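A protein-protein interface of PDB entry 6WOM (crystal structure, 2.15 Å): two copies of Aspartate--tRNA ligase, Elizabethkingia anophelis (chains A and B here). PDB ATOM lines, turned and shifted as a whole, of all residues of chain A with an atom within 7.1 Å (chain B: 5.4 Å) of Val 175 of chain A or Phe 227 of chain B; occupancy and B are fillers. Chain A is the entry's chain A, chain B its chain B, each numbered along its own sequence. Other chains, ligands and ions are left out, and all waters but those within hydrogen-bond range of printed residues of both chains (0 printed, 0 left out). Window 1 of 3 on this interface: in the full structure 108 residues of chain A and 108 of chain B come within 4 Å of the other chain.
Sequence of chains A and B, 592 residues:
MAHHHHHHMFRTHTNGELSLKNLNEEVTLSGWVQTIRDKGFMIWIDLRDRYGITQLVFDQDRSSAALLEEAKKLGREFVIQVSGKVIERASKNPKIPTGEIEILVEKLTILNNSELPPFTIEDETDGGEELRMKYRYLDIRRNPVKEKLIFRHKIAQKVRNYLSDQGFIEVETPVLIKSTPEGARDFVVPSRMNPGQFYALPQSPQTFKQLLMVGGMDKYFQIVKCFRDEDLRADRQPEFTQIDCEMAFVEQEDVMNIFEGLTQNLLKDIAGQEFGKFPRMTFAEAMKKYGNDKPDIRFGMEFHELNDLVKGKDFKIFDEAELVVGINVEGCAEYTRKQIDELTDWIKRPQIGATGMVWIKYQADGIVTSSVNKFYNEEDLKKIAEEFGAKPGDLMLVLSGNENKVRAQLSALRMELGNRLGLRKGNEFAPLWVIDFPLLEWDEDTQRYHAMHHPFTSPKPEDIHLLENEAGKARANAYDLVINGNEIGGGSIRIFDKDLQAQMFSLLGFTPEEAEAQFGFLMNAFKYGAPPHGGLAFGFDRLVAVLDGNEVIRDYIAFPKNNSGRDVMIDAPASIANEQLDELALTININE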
ATOM      1  N   THR A 173      12.644 -22.713 -31.810  1.00  0.00           N
ATOM      2  CA  THR A 173      11.492 -23.548 -31.585  1.00  0.00           C
ATOM      3  C   THR A 173      10.285 -22.664 -31.303  1.00  0.00           C
ATOM      4  O   THR A 173      10.443 -21.485 -30.977  1.00  0.00           O
ATOM      5  CB  THR A 173      11.776 -24.505 -30.418  1.00  0.00           C
ATOM      6  OG1 THR A 173      12.119 -23.751 -29.251  1.00  0.00           O
ATOM      7  CG2 THR A 173      12.977 -25.415 -30.797  1.00  0.00           C
ATOM      8  N   PRO A 174       9.062 -23.170 -31.477  1.00  0.00           N
ATOM      9  CA  PRO A 174       7.897 -22.287 -31.376  1.00  0.00           C
ATOM     10  C   PRO A 174       7.684 -21.725 -29.975  1.00  0.00           C
ATOM     11  O   PRO A 174       8.055 -22.319 -28.962  1.00  0.00           O
ATOM     12  CB  PRO A 174       6.717 -23.189 -31.790  1.00  0.00           C
ATOM     13  CG  PRO A 174       7.319 -24.362 -32.448  1.00  0.00           C
ATOM     14  CD  PRO A 174       8.674 -24.545 -31.832  1.00  0.00           C
ATOM     15  N   VAL A 175       7.064 -20.554 -29.946  1.00  0.00           N
ATOM     16  CA  VAL A 175       6.600 -19.946 -28.715  1.00  0.00           C
ATOM     17  C   VAL A 175       5.136 -20.275 -28.435  1.00  0.00           C
ATOM     18  O   VAL A 175       4.731 -20.383 -27.274  1.00  0.00           O
ATOM     19  CB  VAL A 175       6.833 -18.438 -28.815  1.00  0.00           C
ATOM     20  CG1 VAL A 175       6.195 -17.718 -27.660  1.00  0.00           C
ATOM     21  CG2 VAL A 175       8.354 -18.155 -28.851  1.00  0.00           C
ATOM     22  N   LEU A 176       4.328 -20.449 -29.468  1.00  0.00           N
ATOM     23  CA  LEU A 176       2.923 -20.814 -29.300  1.00  0.00           C
ATOM     24  C   LEU A 176       2.855 -22.335 -29.344  1.00  0.00           C
ATOM     25  O   LEU A 176       2.857 -22.934 -30.422  1.00  0.00           O
ATOM     26  CB  LEU A 176       2.074 -20.198 -30.403  1.00  0.00           C
ATOM     27  CG  LEU A 176       2.152 -18.680 -30.531  1.00  0.00           C
ATOM     28  CD1 LEU A 176       1.374 -18.193 -31.752  1.00  0.00           C
ATOM     29  CD2 LEU A 176       1.630 -18.053 -29.258  1.00  0.00           C
ATOM     30  N   ILE A 177       2.808 -22.980 -28.179  1.00  0.00           N
ATOM     31  CA  ILE A 177       2.833 -24.441 -28.156  1.00  0.00           C
ATOM     32  C   ILE A 177       1.597 -24.976 -27.438  1.00  0.00           C
ATOM     33  O   ILE A 177       0.602 -24.258 -27.266  1.00  0.00           O
ATOM     34  CB  ILE A 177       4.131 -24.952 -27.506  1.00  0.00           C
ATOM     35  CG1 ILE A 177       4.204 -24.524 -26.030  1.00  0.00           C
ATOM     36  CG2 ILE A 177       5.347 -24.418 -28.267  1.00  0.00           C
ATOM     37  CD1 ILE A 177       5.295 -25.213 -25.282  1.00  0.00           C
ATOM     38  N   LYS A 178       1.628 -26.236 -27.022  1.00  0.00           N
ATOM     39  CA  LYS A 178       0.448 -26.847 -26.416  1.00  0.00           C
ATOM     40  C   LYS A 178       0.542 -26.757 -24.893  1.00  0.00           C
ATOM     41  O   LYS A 178       1.587 -27.069 -24.309  1.00  0.00           O
ATOM     42  CB  LYS A 178       0.289 -28.303 -26.857  1.00  0.00           C
ATOM     43  CG  LYS A 178      -0.948 -28.972 -26.296  1.00  0.00           C
ATOM     44  CD  LYS A 178      -1.428 -30.096 -27.206  1.00  0.00           C
ATOM     45  CE  LYS A 178      -2.595 -30.869 -26.600  1.00  0.00           C
ATOM     46  NZ  LYS A 178      -3.474 -31.459 -27.674  1.00  0.00           N
ATOM     47  N   VAL A 189      -2.513 -18.407 -24.224  1.00  0.00           N
ATOM     48  CA  VAL A 189      -2.812 -17.468 -25.305  1.00  0.00           C
ATOM     49  C   VAL A 189      -4.112 -17.904 -25.989  1.00  0.00           C
ATOM     50  O   VAL A 189      -4.117 -18.899 -26.722  1.00  0.00           O
ATOM     51  CB  VAL A 189      -1.661 -17.409 -26.322  1.00  0.00           C
ATOM     52  CG1 VAL A 189      -2.006 -16.460 -27.478  1.00  0.00           C
ATOM     53  CG2 VAL A 189      -0.349 -16.973 -25.634  1.00  0.00           C
ATOM     54  N   TYR A 199      -3.196 -21.624 -26.892  1.00  0.00           N
ATOM     55  CA  TYR A 199      -1.805 -22.029 -26.859  1.00  0.00           C
ATOM     56  C   TYR A 199      -1.273 -21.790 -25.444  1.00  0.00           C
ATOM     57  O   TYR A 199      -1.871 -21.060 -24.644  1.00  0.00           O
ATOM     58  CB  TYR A 199      -0.955 -21.212 -27.829  1.00  0.00           C
ATOM     59  CG  TYR A 199      -1.414 -21.115 -29.278  1.00  0.00           C
ATOM     60  CD1 TYR A 199      -1.041 -22.058 -30.233  1.00  0.00           C
ATOM     61  CD2 TYR A 199      -2.171 -20.028 -29.695  1.00  0.00           C
ATOM     62  CE1 TYR A 199      -1.431 -21.925 -31.570  1.00  0.00           C
ATOM     63  CE2 TYR A 199      -2.565 -19.890 -31.011  1.00  0.00           C
ATOM     64  CZ  TYR A 199      -2.189 -20.831 -31.940  1.00  0.00           C
ATOM     65  OH  TYR A 199      -2.611 -20.672 -33.237  1.00  0.00           O
ATOM     66  N   ALA A 200      -0.114 -22.385 -25.151  1.00  0.00           N
ATOM     67  CA  ALA A 200       0.668 -21.986 -23.998  1.00  0.00           C
ATOM     68  C   ALA A 200       1.997 -21.403 -24.460  1.00  0.00           C
ATOM     69  O   ALA A 200       2.528 -21.781 -25.512  1.00  0.00           O
ATOM     70  CB  ALA A 200       0.925 -23.167 -23.051  1.00  0.00           C
ATOM     71  N   LEU A 201       2.547 -20.471 -23.640  1.00  0.00           N
ATOM     72  CA  LEU A 201       3.933 -20.078 -23.806  1.00  0.00           C
ATOM     73  C   LEU A 201       4.820 -21.159 -23.184  1.00  0.00           C
ATOM     74  O   LEU A 201       4.416 -21.837 -22.233  1.00  0.00           O
ATOM     75  CB  LEU A 201       4.199 -18.725 -23.147  1.00  0.00           C
ATOM     76  CG  LEU A 201       3.260 -17.582 -23.570  1.00  0.00           C
ATOM     77  CD1 LEU A 201       3.724 -16.285 -22.917  1.00  0.00           C
ATOM     78  CD2 LEU A 201       3.178 -17.441 -25.093  1.00  0.00           C
ATOM     79  N   PRO A 202       6.011 -21.378 -23.738  1.00  0.00           N
ATOM     80  CA  PRO A 202       6.820 -22.527 -23.327  1.00  0.00           C
ATOM     81  C   PRO A 202       7.500 -22.301 -21.978  1.00  0.00           C
ATOM     82  O   PRO A 202       8.101 -21.253 -21.727  1.00  0.00           O
ATOM     83  CB  PRO A 202       7.843 -22.661 -24.463  1.00  0.00           C
ATOM     84  CG  PRO A 202       7.955 -21.291 -25.032  1.00  0.00           C
ATOM     85  CD  PRO A 202       6.635 -20.624 -24.845  1.00  0.00           C
ATOM     86  N   PHE A 208      10.465 -29.864 -27.899  1.00  0.00           N
ATOM     87  CA  PHE A 208      11.000 -29.720 -29.246  1.00  0.00           C
ATOM     88  C   PHE A 208      12.474 -30.087 -29.304  1.00  0.00           C
ATOM     89  O   PHE A 208      12.931 -30.637 -30.310  1.00  0.00           O
ATOM     90  CB  PHE A 208      10.741 -28.285 -29.758  1.00  0.00           C
ATOM     91  CG  PHE A 208       9.280 -27.990 -29.923  1.00  0.00           C
ATOM     92  CD1 PHE A 208       8.637 -28.285 -31.108  1.00  0.00           C
ATOM     93  CD2 PHE A 208       8.531 -27.502 -28.862  1.00  0.00           C
ATOM     94  CE1 PHE A 208       7.277 -28.063 -31.248  1.00  0.00           C
ATOM     95  CE2 PHE A 208       7.171 -27.289 -28.992  1.00  0.00           C
ATOM     96  CZ  PHE A 208       6.543 -27.572 -30.192  1.00  0.00           C
ATOM     97  N   GLN A 222      20.065 -23.136 -28.125  1.00  0.00           N
ATOM     98  CA  GLN A 222      19.208 -21.976 -28.280  1.00  0.00           C
ATOM     99  C   GLN A 222      19.381 -21.122 -27.033  1.00  0.00           C
ATOM    100  O   GLN A 222      19.320 -21.655 -25.920  1.00  0.00           O
ATOM    101  CB  GLN A 222      17.747 -22.439 -28.430  1.00  0.00           C
ATOM    102  CG  GLN A 222      16.881 -21.452 -29.094  1.00  0.00           C
ATOM    103  CD  GLN A 222      15.421 -21.867 -29.174  1.00  0.00           C
ATOM    104  OE1 GLN A 222      14.600 -21.061 -29.602  1.00  0.00           O
ATOM    105  NE2 GLN A 222      15.077 -23.104 -28.738  1.00  0.00           N
ATOM    106  N   VAL A 224      17.138 -18.621 -25.312  1.00  0.00           N
ATOM    107  CA  VAL A 224      15.697 -18.622 -25.541  1.00  0.00           C
ATOM    108  C   VAL A 224      14.961 -18.130 -24.299  1.00  0.00           C
ATOM    109  O   VAL A 224      15.345 -18.447 -23.167  1.00  0.00           O
ATOM    110  CB  VAL A 224      15.213 -20.033 -25.959  1.00  0.00           C
ATOM    111  CG1 VAL A 224      15.549 -21.078 -24.871  1.00  0.00           C
ATOM    112  CG2 VAL A 224      13.696 -20.043 -26.251  1.00  0.00           C
ATOM    113  N   LYS A 225      13.903 -17.354 -24.518  1.00  0.00           N
ATOM    114  CA  LYS A 225      13.008 -16.940 -23.443  1.00  0.00           C
ATOM    115  C   LYS A 225      12.120 -18.098 -23.004  1.00  0.00           C
ATOM    116  O   LYS A 225      11.590 -18.845 -23.829  1.00  0.00           O
ATOM    117  CB  LYS A 225      12.119 -15.785 -23.899  1.00  0.00           C
ATOM    118  CG  LYS A 225      12.779 -14.444 -23.878  1.00  0.00           C
ATOM    119  CD  LYS A 225      12.888 -13.907 -22.466  1.00  0.00           C
ATOM    120  CE  LYS A 225      13.400 -12.452 -22.452  1.00  0.00           C
ATOM    121  NZ  LYS A 225      12.399 -11.457 -22.949  1.00  0.00           N
ATOM    122  N   PHE A 227       8.922 -19.072 -19.951  1.00  0.00           N
ATOM    123  CA  PHE A 227       7.811 -18.370 -19.328  1.00  0.00           C
ATOM    124  C   PHE A 227       7.195 -19.265 -18.270  1.00  0.00           C
ATOM    125  O   PHE A 227       6.804 -20.395 -18.569  1.00  0.00           O
ATOM    126  CB  PHE A 227       6.758 -17.973 -20.378  1.00  0.00           C
ATOM    127  CG  PHE A 227       7.313 -17.181 -21.512  1.00  0.00           C
ATOM    128  CD1 PHE A 227       7.937 -17.805 -22.570  1.00  0.00           C
ATOM    129  CD2 PHE A 227       7.203 -15.796 -21.526  1.00  0.00           C
ATOM    130  CE1 PHE A 227       8.464 -17.063 -23.623  1.00  0.00           C
ATOM    131  CE2 PHE A 227       7.717 -15.054 -22.580  1.00  0.00           C
ATOM    132  CZ  PHE A 227       8.353 -15.687 -23.621  1.00  0.00           C
ATOM    133  N   VAL B 175       8.670  -9.944 -23.972  1.00  0.00           N
ATOM    134  CA  VAL B 175       7.635 -10.581 -24.776  1.00  0.00           C
ATOM    135  C   VAL B 175       6.261 -10.286 -24.189  1.00  0.00           C
ATOM    136  O   VAL B 175       5.272 -10.220 -24.925  1.00  0.00           O
ATOM    137  CB  VAL B 175       7.888 -12.094 -24.864  1.00  0.00           C
ATOM    138  CG1 VAL B 175       6.711 -12.806 -25.500  1.00  0.00           C
ATOM    139  CG2 VAL B 175       9.174 -12.392 -25.646  1.00  0.00           C
ATOM    140  N   ARG B 185      -3.937  -6.938 -35.080  1.00  0.00           N
ATOM    141  CA  ARG B 185      -4.487  -7.656 -33.932  1.00  0.00           C
ATOM    142  C   ARG B 185      -3.377  -8.313 -33.111  1.00  0.00           C
ATOM    143  O   ARG B 185      -2.579  -9.089 -33.637  1.00  0.00           O
ATOM    144  CB  ARG B 185      -5.492  -8.704 -34.386  1.00  0.00           C
ATOM    145  CG  ARG B 185      -6.186  -9.422 -33.246  1.00  0.00           C
ATOM    146  CD  ARG B 185      -7.082 -10.516 -33.783  1.00  0.00           C
ATOM    147  NE  ARG B 185      -8.291  -9.970 -34.406  1.00  0.00           N
ATOM    148  CZ  ARG B 185      -8.502  -9.879 -35.719  1.00  0.00           C
ATOM    149  NH1 ARG B 185      -7.588 -10.294 -36.584  1.00  0.00           N
ATOM    150  NH2 ARG B 185      -9.642  -9.376 -36.169  1.00  0.00           N
ATOM    151  N   PHE B 187      -1.982 -11.010 -30.346  1.00  0.00           N
ATOM    152  CA  PHE B 187      -2.198 -12.133 -29.439  1.00  0.00           C
ATOM    153  C   PHE B 187      -2.134 -11.619 -28.002  1.00  0.00           C
ATOM    154  O   PHE B 187      -1.332 -10.733 -27.694  1.00  0.00           O
ATOM    155  CB  PHE B 187      -1.123 -13.215 -29.628  1.00  0.00           C
ATOM    156  CG  PHE B 187      -1.302 -14.051 -30.856  1.00  0.00           C
ATOM    157  CD1 PHE B 187      -2.300 -15.014 -30.911  1.00  0.00           C
ATOM    158  CD2 PHE B 187      -0.450 -13.904 -31.950  1.00  0.00           C
ATOM    159  CE1 PHE B 187      -2.469 -15.810 -32.051  1.00  0.00           C
ATOM    160  CE2 PHE B 187      -0.612 -14.696 -33.095  1.00  0.00           C
ATOM    161  CZ  PHE B 187      -1.615 -15.644 -33.139  1.00  0.00           C
ATOM    162  N   LEU B 201       1.480 -10.151 -26.788  1.00  0.00           N
ATOM    163  CA  LEU B 201       2.736 -10.529 -27.408  1.00  0.00           C
ATOM    164  C   LEU B 201       3.115  -9.455 -28.431  1.00  0.00           C
ATOM    165  O   LEU B 201       2.242  -8.848 -29.060  1.00  0.00           O
ATOM    166  CB  LEU B 201       2.621 -11.896 -28.081  1.00  0.00           C
ATOM    167  CG  LEU B 201       2.116 -13.022 -27.163  1.00  0.00           C
ATOM    168  CD1 LEU B 201       2.122 -14.343 -27.931  1.00  0.00           C
ATOM    169  CD2 LEU B 201       2.967 -13.151 -25.887  1.00  0.00           C
ATOM    170  N   PRO B 202       4.407  -9.187 -28.602  1.00  0.00           N
ATOM    171  CA  PRO B 202       4.810  -8.021 -29.401  1.00  0.00           C
ATOM    172  C   PRO B 202       4.669  -8.289 -30.895  1.00  0.00           C
ATOM    173  O   PRO B 202       5.045  -9.357 -31.383  1.00  0.00           O
ATOM    174  CB  PRO B 202       6.278  -7.796 -28.990  1.00  0.00           C
ATOM    175  CG  PRO B 202       6.758  -9.155 -28.552  1.00  0.00           C
ATOM    176  CD  PRO B 202       5.550  -9.884 -27.999  1.00  0.00           C
ATOM    177  N   GLN B 203       4.092  -7.320 -31.614  1.00  0.00           N
ATOM    178  CA  GLN B 203       4.176  -7.335 -33.078  1.00  0.00           C
ATOM    179  C   GLN B 203       5.598  -7.092 -33.557  1.00  0.00           C
ATOM    180  O   GLN B 203       5.967  -7.535 -34.656  1.00  0.00           O
ATOM    181  CB  GLN B 203       3.283  -6.252 -33.710  1.00  0.00           C
ATOM    182  CG  GLN B 203       1.894  -6.192 -33.159  1.00  0.00           C
ATOM    183  CD  GLN B 203       0.924  -6.964 -34.016  1.00  0.00           C
ATOM    184  OE1 GLN B 203       1.244  -7.351 -35.141  1.00  0.00           O
ATOM    185  NE2 GLN B 203      -0.251  -7.244 -33.467  1.00  0.00           N
ATOM    186  N   LYS B 225      11.604 -12.930 -32.295  1.00  0.00           N
ATOM    187  CA  LYS B 225      10.282 -13.406 -32.659  1.00  0.00           C
ATOM    188  C   LYS B 225       9.251 -12.302 -32.510  1.00  0.00           C
ATOM    189  O   LYS B 225       9.271 -11.537 -31.538  1.00  0.00           O
ATOM    190  CB  LYS B 225       9.846 -14.587 -31.776  1.00  0.00           C
ATOM    191  CG  LYS B 225      10.418 -15.910 -32.190  1.00  0.00           C
ATOM    192  CD  LYS B 225       9.763 -16.425 -33.461  1.00  0.00           C
ATOM    193  CE  LYS B 225      10.190 -17.869 -33.743  1.00  0.00           C
ATOM    194  NZ  LYS B 225       9.557 -18.811 -32.788  1.00  0.00           N
ATOM    195  N   CYS B 226       8.340 -12.250 -33.477  1.00  0.00           N
ATOM    196  CA  CYS B 226       7.221 -11.326 -33.519  1.00  0.00           C
ATOM    197  C   CYS B 226       5.941 -12.118 -33.716  1.00  0.00           C
ATOM    198  O   CYS B 226       5.952 -13.237 -34.232  1.00  0.00           O
ATOM    199  CB  CYS B 226       7.381 -10.319 -34.666  1.00  0.00           C
ATOM    200  SG  CYS B 226       8.956  -9.439 -34.610  1.00  0.00           S
ATOM    201  N   PHE B 227       4.827 -11.527 -33.309  1.00  0.00           N
ATOM    202  CA  PHE B 227       3.574 -12.261 -33.245  1.00  0.00           C
ATOM    203  C   PHE B 227       2.446 -11.412 -33.815  1.00  0.00           C
ATOM    204  O   PHE B 227       2.283 -10.255 -33.420  1.00  0.00           O
ATOM    205  CB  PHE B 227       3.269 -12.661 -31.794  1.00  0.00           C
ATOM    206  CG  PHE B 227       4.392 -13.419 -31.122  1.00  0.00           C
ATOM    207  CD1 PHE B 227       5.460 -12.747 -30.528  1.00  0.00           C
ATOM    208  CD2 PHE B 227       4.371 -14.818 -31.076  1.00  0.00           C
ATOM    209  CE1 PHE B 227       6.489 -13.465 -29.900  1.00  0.00           C
ATOM    210  CE2 PHE B 227       5.385 -15.537 -30.453  1.00  0.00           C
ATOM    211  CZ  PHE B 227       6.452 -14.856 -29.861  1.00  0.00           C
ATOM    212  N   ARG B 228       1.665 -11.977 -34.724  1.00  0.00           N
ATOM    213  CA  ARG B 228       0.562 -11.225 -35.313  1.00  0.00           C
ATOM    214  C   ARG B 228      -0.611 -12.169 -35.529  1.00  0.00           C
ATOM    215  O   ARG B 228      -0.446 -13.221 -36.145  1.00  0.00           O
ATOM    216  CB  ARG B 228       0.951 -10.597 -36.657  1.00  0.00           C
ATOM    217  CG  ARG B 228      -0.011  -9.500 -37.096  1.00  0.00           C
ATOM    218  CD  ARG B 228       0.379  -8.853 -38.425  1.00  0.00           C
ATOM    219  NE  ARG B 228       1.677  -8.189 -38.431  1.00  0.00           N
ATOM    220  CZ  ARG B 228       2.629  -8.421 -39.335  1.00  0.00           C
ATOM    221  NH1 ARG B 228       2.430  -9.313 -40.301  1.00  0.00           N
ATOM    222  NH2 ARG B 228       3.781  -7.758 -39.268  1.00  0.00           N
ATOM    223  N   ASP B 229      -1.784 -11.801 -35.023  1.00  0.00           N
ATOM    224  CA  ASP B 229      -2.958 -12.664 -35.137  1.00  0.00           C
ATOM    225  C   ASP B 229      -3.869 -12.116 -36.239  1.00  0.00           C
ATOM    226  O   ASP B 229      -4.962 -11.615 -36.009  1.00  0.00           O
ATOM    227  CB  ASP B 229      -3.675 -12.755 -33.792  1.00  0.00           C
ATOM    228  CG  ASP B 229      -4.828 -13.751 -33.801  1.00  0.00           C
ATOM    229  OD1 ASP B 229      -5.681 -13.674 -32.876  1.00  0.00           O
ATOM    230  OD2 ASP B 229      -4.875 -14.605 -34.725  1.00  0.00           O
ATOM    231  N   PRO B 238       1.838 -17.197 -37.817  1.00  0.00           N
ATOM    232  CA  PRO B 238       1.427 -16.314 -36.708  1.00  0.00           C
ATOM    233  C   PRO B 238       2.598 -15.809 -35.869  1.00  0.00           C
ATOM    234  O   PRO B 238       2.465 -14.776 -35.203  1.00  0.00           O
ATOM    235  CB  PRO B 238       0.477 -17.198 -35.882  1.00  0.00           C
ATOM    236  CG  PRO B 238       0.890 -18.600 -36.204  1.00  0.00           C
ATOM    237  CD  PRO B 238       1.333 -18.576 -37.645  1.00  0.00           C
ATOM    238  N   GLU B 239       3.716 -16.518 -35.861  1.00  0.00           N
ATOM    239  CA  GLU B 239       4.938 -16.056 -35.247  1.00  0.00           C
ATOM    240  C   GLU B 239       6.038 -16.139 -36.290  1.00  0.00           C
ATOM    241  O   GLU B 239       6.077 -17.080 -37.088  1.00  0.00           O
ATOM    242  CB  GLU B 239       5.290 -16.863 -33.954  1.00  0.00           C
ATOM    243  CG  GLU B 239       5.676 -18.311 -34.138  1.00  0.00           C
ATOM    244  CD  GLU B 239       5.874 -19.046 -32.806  1.00  0.00           C
ATOM    245  OE1 GLU B 239       6.963 -18.932 -32.219  1.00  0.00           O
ATOM    246  OE2 GLU B 239       4.948 -19.734 -32.351  1.00  0.00           O
ATOM    247  N   PHE B 240       6.922 -15.135 -36.285  1.00  0.00           N
ATOM    248  CA  PHE B 240       7.902 -14.975 -37.353  1.00  0.00           C
ATOM    249  C   PHE B 240       9.083 -14.203 -36.790  1.00  0.00           C
ATOM    250  O   PHE B 240       8.990 -13.583 -35.730  1.00  0.00           O
ATOM    251  CB  PHE B 240       7.305 -14.256 -38.587  1.00  0.00           C
ATOM    252  CG  PHE B 240       6.689 -12.909 -38.268  1.00  0.00           C
ATOM    253  CD1 PHE B 240       5.392 -12.812 -37.803  1.00  0.00           C
ATOM    254  CD2 PHE B 240       7.418 -11.741 -38.438  1.00  0.00           C
ATOM    255  CE1 PHE B 240       4.839 -11.580 -37.502  1.00  0.00           C
ATOM    256  CE2 PHE B 240       6.871 -10.499 -38.140  1.00  0.00           C
ATOM    257  CZ  PHE B 240       5.583 -10.414 -37.674  1.00  0.00           C
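Among the printed residues, merely in contact across the chains: Pro 174 of chain A with Glu 239 of chain B (3.6 Å), Val 175 of chain A with Phe 227 of chain B (3.6 Å), Leu 176 of chain A with Leu 201 of chain B (3.97 Å), Val 189 of chain A with Phe 187 of chain B (3.7 Å) and Phe 227 of chain A with Val 175 of chain B (3.7 Å).
Val 175 of chain A touches Phe 227 of chain B, and with the chains exchanged Phe 227 of chain A touches Val 175 of chain B.
Of the 8 pairs that touch across the chains among the printed residues, 2 have their exchanged pair printed and touching as well.
O of Thr 173 of chain A lies within hydrogen-bond range of NZ of Lys 225 of chain B, at 3.3 Å.
The backbone NH (N) of Val 175 of chain A lies within hydrogen-bond range of the side-chain carboxylate (OE1) of Glu 239 of chain B.
OE2 of Glu 239 of chain B sits at hydrogen-bond distance from N of Leu 176 of chain A, 3.0 Å away.
The side-chain amide nitrogen (NE2) of Gln 222 of chain A is in hydrogen-bond range of the side-chain hydroxyl (OG1) of Thr 173 of chain A, 3.1 Å away.
O of Tyr 199 of chain A sits at hydrogen-bond distance from N of Val 189 of chain A (2.8 Å).
N of Phe 227 of chain A lies within hydrogen-bond range of O of Pro 202 of chain A (2.9 Å).
O of Phe 187 of chain B sits at hydrogen-bond distance from N of Leu 201 of chain B (3.0 Å).
The backbone carbonyl oxygen (O) of Pro 202 of chain B lies within hydrogen-bond range of the backbone NH (N) of Phe 227 of chain B, at 2.9 Å.
The side-chain carboxylate (OE1) of Glu 239 of chain B is in salt-bridge range of the side-chain amino group (NZ) of Lys 225 of chain B.
Of chain B, only Phe 227 (3.6 Å) and Glu 239 (2.8 Å) come within 4 Å of Val 175 of chain A.
Printed residues of chain B within 4 Å of Val 189 of chain A: Phe 187 (3.7 Å).
Printed residues of chain A within 4 Å of Phe 187 of chain B: Val 189 (3.7 Å).
Of the printed residues of chain B, Leu 176 of chain A touches Leu 201 (3.97 Å) and Glu 239 (3.0 Å).
Lys 178 of chain A touches none of the printed residues of chain B.
The nearest residue of chain B that does not touch Val 175 of chain A is Lys 225 of chain B (4.2 Å).
The nearest printed residue of chain A that does not touch Val 175 of chain B is Lys 225 of chain A (4.2 Å).
Of the 16 printed residues of chain A, 6 touch a printed residue of chain B.
Hydrophobic or aromatic side chains of chain A that line the printed part of chain B: Pro 174, Val 175, Leu 176, Val 189 and Phe 227.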
